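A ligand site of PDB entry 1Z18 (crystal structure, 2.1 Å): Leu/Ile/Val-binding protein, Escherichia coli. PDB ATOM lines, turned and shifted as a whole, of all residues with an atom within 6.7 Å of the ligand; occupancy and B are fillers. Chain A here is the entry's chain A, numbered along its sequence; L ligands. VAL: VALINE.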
ATOM      1  N   TYR A  18       6.722 -16.597  -2.628  1.00  0.00           N
ATOM      2  CA  TYR A  18       5.680 -17.630  -2.480  1.00  0.00           C
ATOM      3  C   TYR A  18       4.367 -16.948  -2.084  1.00  0.00           C
ATOM      4  O   TYR A  18       3.290 -17.302  -2.558  1.00  0.00           O
ATOM      5  CB  TYR A  18       6.052 -18.658  -1.389  1.00  0.00           C
ATOM      6  CG  TYR A  18       7.276 -19.509  -1.683  1.00  0.00           C
ATOM      7  CD1 TYR A  18       7.713 -19.707  -3.005  1.00  0.00           C
ATOM      8  CD2 TYR A  18       8.037 -20.073  -0.658  1.00  0.00           C
ATOM      9  CE1 TYR A  18       8.861 -20.435  -3.283  1.00  0.00           C
ATOM     10  CE2 TYR A  18       9.188 -20.799  -0.922  1.00  0.00           C
ATOM     11  CZ  TYR A  18       9.590 -20.972  -2.242  1.00  0.00           C
ATOM     12  OH  TYR A  18      10.705 -21.691  -2.551  1.00  0.00           O
ATOM     13  N   CYS A  53       7.153 -17.586   6.592  1.00  0.00           N
ATOM     14  CA  CYS A  53       7.594 -18.964   6.343  1.00  0.00           C
ATOM     15  C   CYS A  53       8.606 -19.360   7.415  1.00  0.00           C
ATOM     16  O   CYS A  53       9.580 -20.075   7.150  1.00  0.00           O
ATOM     17  CB  CYS A  53       8.217 -19.141   4.946  1.00  0.00           C
ATOM     18  SG  CYS A  53       7.101 -19.949   3.726  1.00  0.00           S
ATOM     19  N   HIS A  76      -0.670 -22.751   5.491  1.00  0.00           N
ATOM     20  CA  HIS A  76       0.419 -21.849   5.165  1.00  0.00           C
ATOM     21  C   HIS A  76       1.112 -22.422   3.921  1.00  0.00           C
ATOM     22  O   HIS A  76       0.540 -23.268   3.258  1.00  0.00           O
ATOM     23  CB  HIS A  76       1.355 -21.751   6.385  1.00  0.00           C
ATOM     24  CG  HIS A  76       0.651 -21.323   7.642  1.00  0.00           C
ATOM     25  ND1 HIS A  76       1.288 -20.661   8.677  1.00  0.00           N
ATOM     26  CD2 HIS A  76      -0.649 -21.433   8.017  1.00  0.00           C
ATOM     27  CE1 HIS A  76       0.413 -20.382   9.617  1.00  0.00           C
ATOM     28  NE2 HIS A  76      -0.768 -20.848   9.245  1.00  0.00           N
ATOM     29  N   LEU A  77       2.310 -21.953   3.606  1.00  0.00           N
ATOM     30  CA  LEU A  77       3.028 -22.407   2.416  1.00  0.00           C
ATOM     31  C   LEU A  77       4.190 -23.369   2.619  1.00  0.00           C
ATOM     32  O   LEU A  77       4.214 -24.446   2.023  1.00  0.00           O
ATOM     33  CB  LEU A  77       3.535 -21.215   1.598  1.00  0.00           C
ATOM     34  CG  LEU A  77       2.580 -20.292   0.843  1.00  0.00           C
ATOM     35  CD1 LEU A  77       1.274 -20.962   0.417  1.00  0.00           C
ATOM     36  CD2 LEU A  77       2.314 -19.149   1.722  1.00  0.00           C
ATOM     37  N   CYS A  78       5.224 -22.942   3.412  1.00  0.00           N
ATOM     38  CA  CYS A  78       6.398 -23.791   3.665  1.00  0.00           C
ATOM     39  C   CYS A  78       5.969 -24.898   4.612  1.00  0.00           C
ATOM     40  O   CYS A  78       5.134 -24.697   5.492  1.00  0.00           O
ATOM     41  CB  CYS A  78       7.550 -22.949   4.254  1.00  0.00           C
ATOM     42  SG  CYS A  78       8.122 -21.631   3.127  1.00  0.00           S
ATOM     43  N   SER A  79       6.529 -26.087   4.406  1.00  0.00           N
ATOM     44  CA  SER A  79       6.172 -27.222   5.255  1.00  0.00           C
ATOM     45  C   SER A  79       6.580 -27.108   6.726  1.00  0.00           C
ATOM     46  O   SER A  79       5.759 -27.339   7.614  1.00  0.00           O
ATOM     47  CB  SER A  79       6.708 -28.523   4.655  1.00  0.00           C
ATOM     48  OG  SER A  79       5.899 -28.919   3.558  1.00  0.00           O
ATOM     49  N   SER A  80       7.823 -26.729   6.998  1.00  0.00           N
ATOM     50  CA  SER A  80       8.238 -26.657   8.394  1.00  0.00           C
ATOM     51  C   SER A  80       7.512 -25.552   9.181  1.00  0.00           C
ATOM     52  O   SER A  80       7.492 -25.562  10.399  1.00  0.00           O
ATOM     53  CB  SER A  80       9.763 -26.509   8.492  1.00  0.00           C
ATOM     54  OG  SER A  80      10.220 -25.260   8.042  1.00  0.00           O
ATOM     55  N   THR A  82       4.257 -24.778   8.187  1.00  0.00           N
ATOM     56  CA  THR A  82       2.865 -25.257   8.179  1.00  0.00           C
ATOM     57  C   THR A  82       2.603 -26.346   9.264  1.00  0.00           C
ATOM     58  O   THR A  82       1.525 -26.376   9.877  1.00  0.00           O
ATOM     59  CB  THR A  82       2.465 -25.786   6.774  1.00  0.00           C
ATOM     60  OG1 THR A  82       2.506 -24.721   5.808  1.00  0.00           O
ATOM     61  CG2 THR A  82       1.053 -26.302   6.777  1.00  0.00           C
ATOM     62  N   PRO A  99      -2.115 -24.626  -0.153  1.00  0.00           N
ATOM     63  CA  PRO A  99      -1.897 -24.613  -1.598  1.00  0.00           C
ATOM     64  C   PRO A  99      -0.454 -24.785  -1.982  1.00  0.00           C
ATOM     65  O   PRO A  99      -0.088 -24.610  -3.152  1.00  0.00           O
ATOM     66  CB  PRO A  99      -2.400 -23.244  -1.988  1.00  0.00           C
ATOM     67  CG  PRO A  99      -1.845 -22.422  -0.854  1.00  0.00           C
ATOM     68  CD  PRO A  99      -2.207 -23.250   0.360  1.00  0.00           C
ATOM     69  N   ALA A 100       0.404 -25.132  -1.040  1.00  0.00           N
ATOM     70  CA  ALA A 100       1.805 -25.234  -1.428  1.00  0.00           C
ATOM     71  C   ALA A 100       2.637 -26.223  -0.649  1.00  0.00           C
ATOM     72  O   ALA A 100       3.640 -26.715  -1.174  1.00  0.00           O
ATOM     73  CB  ALA A 100       2.449 -23.866  -1.331  1.00  0.00           C
ATOM     74  N   ALA A 101       2.234 -26.515   0.586  1.00  0.00           N
ATOM     75  CA  ALA A 101       3.000 -27.473   1.417  1.00  0.00           C
ATOM     76  C   ALA A 101       2.931 -28.878   0.820  1.00  0.00           C
ATOM     77  O   ALA A 101       1.835 -29.426   0.672  1.00  0.00           O
ATOM     78  CB  ALA A 101       2.469 -27.463   2.853  1.00  0.00           C
ATOM     79  N   THR A 102       4.094 -29.449   0.525  1.00  0.00           N
ATOM     80  CA  THR A 102       4.210 -30.755  -0.108  1.00  0.00           C
ATOM     81  C   THR A 102       4.853 -31.920   0.692  1.00  0.00           C
ATOM     82  O   THR A 102       4.811 -33.078   0.243  1.00  0.00           O
ATOM     83  CB  THR A 102       5.012 -30.627  -1.444  1.00  0.00           C
ATOM     84  OG1 THR A 102       6.337 -30.124  -1.161  1.00  0.00           O
ATOM     85  CG2 THR A 102       4.308 -29.677  -2.397  1.00  0.00           C
ATOM     86  N   ALA A 103       5.450 -31.648   1.843  1.00  0.00           N
ATOM     87  CA  ALA A 103       6.058 -32.738   2.608  1.00  0.00           C
ATOM     88  C   ALA A 103       4.959 -33.715   3.016  1.00  0.00           C
ATOM     89  O   ALA A 103       3.864 -33.324   3.424  1.00  0.00           O
ATOM     90  CB  ALA A 103       6.782 -32.209   3.846  1.00  0.00           C
ATOM     91  N   ARG A 116      -4.971 -30.410   0.862  1.00  0.00           N
ATOM     92  CA  ARG A 116      -3.970 -29.734   0.031  1.00  0.00           C
ATOM     93  C   ARG A 116      -4.561 -29.522  -1.357  1.00  0.00           C
ATOM     94  O   ARG A 116      -5.430 -30.289  -1.779  1.00  0.00           O
ATOM     95  CB  ARG A 116      -2.698 -30.571  -0.181  1.00  0.00           C
ATOM     96  CG  ARG A 116      -2.185 -31.398   0.997  1.00  0.00           C
ATOM     97  CD  ARG A 116      -0.692 -31.726   0.836  1.00  0.00           C
ATOM     98  NE  ARG A 116      -0.238 -32.796   1.726  1.00  0.00           N
ATOM     99  CZ  ARG A 116       0.969 -32.875   2.272  1.00  0.00           C
ATOM    100  NH1 ARG A 116       1.272 -33.904   3.062  1.00  0.00           N
ATOM    101  NH2 ARG A 116       1.886 -31.957   2.032  1.00  0.00           N
ATOM    102  N   THR A 118      -2.226 -29.075  -3.744  1.00  0.00           N
ATOM    103  CA  THR A 118      -0.963 -29.330  -4.427  1.00  0.00           C
ATOM    104  C   THR A 118      -0.606 -30.774  -4.139  1.00  0.00           C
ATOM    105  O   THR A 118      -1.292 -31.436  -3.356  1.00  0.00           O
ATOM    106  CB  THR A 118       0.159 -28.424  -3.953  1.00  0.00           C
ATOM    107  OG1 THR A 118       1.333 -28.679  -4.734  1.00  0.00           O
ATOM    108  CG2 THR A 118       0.460 -28.667  -2.526  1.00  0.00           C
ATOM    109  N   ASP A 121       5.628 -34.724  -2.031  1.00  0.00           N
ATOM    110  CA  ASP A 121       6.993 -34.912  -2.476  1.00  0.00           C
ATOM    111  C   ASP A 121       7.273 -36.401  -2.648  1.00  0.00           C
ATOM    112  O   ASP A 121       8.280 -36.791  -3.214  1.00  0.00           O
ATOM    113  CB  ASP A 121       7.981 -34.234  -1.534  1.00  0.00           C
ATOM    114  CG  ASP A 121       7.803 -32.712  -1.515  1.00  0.00           C
ATOM    115  OD1 ASP A 121       7.655 -32.121  -2.604  1.00  0.00           O
ATOM    116  OD2 ASP A 121       7.817 -32.101  -0.431  1.00  0.00           O
ATOM    117  N   GLN A 124       6.703 -36.012  -6.181  1.00  0.00           N
ATOM    118  CA  GLN A 124       7.648 -35.081  -6.805  1.00  0.00           C
ATOM    119  C   GLN A 124       9.078 -35.630  -6.860  1.00  0.00           C
ATOM    120  O   GLN A 124       9.739 -35.533  -7.888  1.00  0.00           O
ATOM    121  CB  GLN A 124       7.624 -33.723  -6.098  1.00  0.00           C
ATOM    122  CG  GLN A 124       8.410 -32.706  -6.887  1.00  0.00           C
ATOM    123  CD  GLN A 124       8.226 -31.262  -6.418  1.00  0.00           C
ATOM    124  OE1 GLN A 124       8.593 -30.332  -7.137  1.00  0.00           O
ATOM    125  NE2 GLN A 124       7.674 -31.084  -5.244  1.00  0.00           N
ATOM    126  N   GLN A 148      16.465 -28.668   5.574  1.00  0.00           N
ATOM    127  CA  GLN A 148      15.110 -28.373   6.005  1.00  0.00           C
ATOM    128  C   GLN A 148      14.218 -29.518   5.517  1.00  0.00           C
ATOM    129  O   GLN A 148      14.537 -30.207   4.552  1.00  0.00           O
ATOM    130  CB  GLN A 148      14.671 -27.055   5.383  1.00  0.00           C
ATOM    131  CG  GLN A 148      13.394 -26.447   5.887  1.00  0.00           C
ATOM    132  CD  GLN A 148      13.224 -25.013   5.399  1.00  0.00           C
ATOM    133  OE1 GLN A 148      12.130 -24.437   5.450  1.00  0.00           O
ATOM    134  NE2 GLN A 148      14.335 -24.412   4.939  1.00  0.00           N
ATOM    135  N   GLN A 149      13.114 -29.714   6.225  1.00  0.00           N
ATOM    136  CA  GLN A 149      12.126 -30.741   5.964  1.00  0.00           C
ATOM    137  C   GLN A 149      11.811 -31.032   4.491  1.00  0.00           C
ATOM    138  O   GLN A 149      11.867 -32.174   4.032  1.00  0.00           O
ATOM    139  CB  GLN A 149      10.842 -30.335   6.683  1.00  0.00           C
ATOM    140  CG  GLN A 149       9.780 -31.375   6.720  1.00  0.00           C
ATOM    141  CD  GLN A 149       8.587 -30.922   7.520  1.00  0.00           C
ATOM    142  OE1 GLN A 149       8.693 -30.577   8.699  1.00  0.00           O
ATOM    143  NE2 GLN A 149       7.431 -30.903   6.878  1.00  0.00           N
ATOM    144  N   TYR A 150      11.428 -29.987   3.767  1.00  0.00           N
ATOM    145  CA  TYR A 150      11.095 -30.067   2.369  1.00  0.00           C
ATOM    146  C   TYR A 150      12.282 -30.468   1.494  1.00  0.00           C
ATOM    147  O   TYR A 150      12.182 -31.400   0.700  1.00  0.00           O
ATOM    148  CB  TYR A 150      10.549 -28.707   1.924  1.00  0.00           C
ATOM    149  CG  TYR A 150      10.394 -28.511   0.438  1.00  0.00           C
ATOM    150  CD1 TYR A 150       9.322 -29.076  -0.256  1.00  0.00           C
ATOM    151  CD2 TYR A 150      11.295 -27.709  -0.270  1.00  0.00           C
ATOM    152  CE1 TYR A 150       9.149 -28.862  -1.624  1.00  0.00           C
ATOM    153  CE2 TYR A 150      11.135 -27.485  -1.643  1.00  0.00           C
ATOM    154  CZ  TYR A 150      10.053 -28.063  -2.310  1.00  0.00           C
ATOM    155  OH  TYR A 150       9.873 -27.849  -3.655  1.00  0.00           O
ATOM    156  N   GLY A 151      13.408 -29.761   1.651  1.00  0.00           N
ATOM    157  CA  GLY A 151      14.594 -30.031   0.848  1.00  0.00           C
ATOM    158  C   GLY A 151      15.305 -31.341   1.094  1.00  0.00           C
ATOM    159  O   GLY A 151      15.750 -32.019   0.165  1.00  0.00           O
ATOM    160  N   GLY A 201      15.555 -27.704  -2.208  1.00  0.00           N
ATOM    161  CA  GLY A 201      15.432 -26.523  -1.381  1.00  0.00           C
ATOM    162  C   GLY A 201      14.684 -25.403  -2.084  1.00  0.00           C
ATOM    163  O   GLY A 201      13.947 -25.653  -3.025  1.00  0.00           O
ATOM    164  N   TYR A 202      14.893 -24.159  -1.621  1.00  0.00           N
ATOM    165  CA  TYR A 202      14.258 -22.943  -2.138  1.00  0.00           C
ATOM    166  C   TYR A 202      15.124 -22.109  -3.064  1.00  0.00           C
ATOM    167  O   TYR A 202      16.334 -22.269  -3.070  1.00  0.00           O
ATOM    168  CB  TYR A 202      13.811 -22.061  -0.959  1.00  0.00           C
ATOM    169  CG  TYR A 202      12.829 -22.764  -0.024  1.00  0.00           C
ATOM    170  CD1 TYR A 202      11.958 -23.741  -0.510  1.00  0.00           C
ATOM    171  CD2 TYR A 202      12.714 -22.388   1.307  1.00  0.00           C
ATOM    172  CE1 TYR A 202      10.991 -24.338   0.315  1.00  0.00           C
ATOM    173  CE2 TYR A 202      11.754 -22.965   2.134  1.00  0.00           C
ATOM    174  CZ  TYR A 202      10.893 -23.934   1.630  1.00  0.00           C
ATOM    175  OH  TYR A 202       9.913 -24.464   2.438  1.00  0.00           O
ATOM    176  N   GLU A 226       9.739 -27.716  -7.346  1.00  0.00           N
ATOM    177  CA  GLU A 226       8.927 -26.570  -7.702  1.00  0.00           C
ATOM    178  C   GLU A 226       9.324 -25.351  -6.878  1.00  0.00           C
ATOM    179  O   GLU A 226       9.077 -24.206  -7.282  1.00  0.00           O
ATOM    180  CB  GLU A 226       7.436 -26.881  -7.536  1.00  0.00           C
ATOM    181  CG  GLU A 226       6.734 -26.306  -6.290  1.00  0.00           C
ATOM    182  CD  GLU A 226       6.999 -27.089  -5.022  1.00  0.00           C
ATOM    183  OE1 GLU A 226       6.428 -26.708  -3.969  1.00  0.00           O
ATOM    184  OE2 GLU A 226       7.754 -28.074  -5.066  1.00  0.00           O
ATOM    185  N   GLY A 227       9.976 -25.578  -5.736  1.00  0.00           N
ATOM    186  CA  GLY A 227      10.402 -24.486  -4.873  1.00  0.00           C
ATOM    187  C   GLY A 227      11.389 -23.511  -5.513  1.00  0.00           C
ATOM    188  O   GLY A 227      11.544 -22.378  -5.040  1.00  0.00           O
ATOM    189  N   VAL A 228      12.083 -23.936  -6.578  1.00  0.00           N
ATOM    190  CA  VAL A 228      13.039 -23.048  -7.241  1.00  0.00           C
ATOM    191  C   VAL A 228      12.493 -22.493  -8.560  1.00  0.00           C
ATOM    192  O   VAL A 228      13.119 -21.628  -9.191  1.00  0.00           O
ATOM    193  CB  VAL A 228      14.400 -23.769  -7.529  1.00  0.00           C
ATOM    194  CG1 VAL A 228      15.045 -24.225  -6.249  1.00  0.00           C
ATOM    195  CG2 VAL A 228      14.206 -24.953  -8.477  1.00  0.00           C
ATOM    196  N   PHE A 276       1.456 -21.188  -7.620  1.00  0.00           N
ATOM    197  CA  PHE A 276       0.664 -20.914  -6.418  1.00  0.00           C
ATOM    198  C   PHE A 276      -0.498 -19.951  -6.620  1.00  0.00           C
ATOM    199  O   PHE A 276      -1.400 -19.872  -5.786  1.00  0.00           O
ATOM    200  CB  PHE A 276       1.570 -20.465  -5.270  1.00  0.00           C
ATOM    201  CG  PHE A 276       2.659 -21.458  -4.936  1.00  0.00           C
ATOM    202  CD1 PHE A 276       2.443 -22.819  -5.083  1.00  0.00           C
ATOM    203  CD2 PHE A 276       3.906 -21.032  -4.468  1.00  0.00           C
ATOM    204  CE1 PHE A 276       3.432 -23.751  -4.761  1.00  0.00           C
ATOM    205  CE2 PHE A 276       4.908 -21.959  -4.142  1.00  0.00           C
ATOM    206  CZ  PHE A 276       4.670 -23.322  -4.291  1.00  0.00           C
HETATM  207  N   VAL L   1       6.409 -27.026  -1.342  1.00  0.00           N
HETATM  208  CA  VAL L   1       7.413 -26.304  -0.515  1.00  0.00           C
HETATM  209  C   VAL L   1       7.256 -26.680   0.961  1.00  0.00           C
HETATM  210  O   VAL L   1       7.929 -26.091   1.833  1.00  0.00           O
HETATM  211  CB  VAL L   1       7.286 -24.745  -0.719  1.00  0.00           C
HETATM  212  CG1 VAL L   1       7.762 -24.360  -2.141  1.00  0.00           C
HETATM  213  CG2 VAL L   1       5.868 -24.315  -0.549  1.00  0.00           C
HETATM  214  OXT VAL L   1       6.421 -27.585   1.226  1.00  0.00           O
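The side-chain hydroxyl (OH) of Tyr 202 is in hydrogen-bond range of an oxygen (O) of the ligand. A nitrogen (N) of the ligand is in salt-bridge range of the side-chain carboxylate (OE1) of Glu 226, at 2.6 Å. The backbone NH (N) of Ser 79 sits at hydrogen-bond distance from an oxygen (O) of the ligand (2.9 Å). The side-chain hydroxyl (OG) of Ser 79 is in hydrogen-bond range of an oxygen (OXT) of the ligand (2.7 Å). N of the ligand is in hydrogen-bond range of O of Ala 100. An oxygen (OXT) of the ligand lies within hydrogen-bond range of the backbone NH (N) of Thr 102. The side-chain hydroxyl of Thr 102 sits at hydrogen-bond distance from a nitrogen (N) of the ligand, at 3.1 Å.
OH of Tyr 202 lies close to SG of Cys 78, 3.4 Å away. The side-chain carboxylate (OE2) of Glu 226 lies within hydrogen-bond range of the side-chain hydroxyl (OH) of Tyr 150 (2.6 Å). The side-chain amide oxygen (OE1) of Gln 124 sits at hydrogen-bond distance from the backbone NH (N) of Glu 226 (2.9 Å). The backbone NH of Ala 103 is in hydrogen-bond range of the side-chain hydroxyl of Ser 79, at 3.3 Å. The backbone carbonyl oxygen (O) of Leu 77 is in hydrogen-bond range of the backbone NH (N) of Ala 101 (3.2 Å). OD2 of Asp 121 lies within hydrogen-bond range of OG1 of Thr 102. N of Gly 227 lies within hydrogen-bond range of OH of Tyr 150, 3.1 Å away. NH2 of Arg 116 lies within hydrogen-bond range of O of Ala 101, 2.9 Å away.
Tyr 18 touches the ligand. Leu 77 touches the ligand. Cys 78 touches the ligand (CA to O, 3.3 Å). Ala 101 touches the ligand. Tyr 150 touches the ligand. CA of Gly 227 touches CG1 of the ligand, 3.8 Å away. Phe 276 touches the ligand. 12 residues have an atom within 4 Å of the ligand: Tyr 18, Leu 77, Cys 78, Ser 79, Ala 100, Ala 101, Thr 102, Tyr 150, Tyr 202, Glu 226, Gly 227 and Phe 276.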
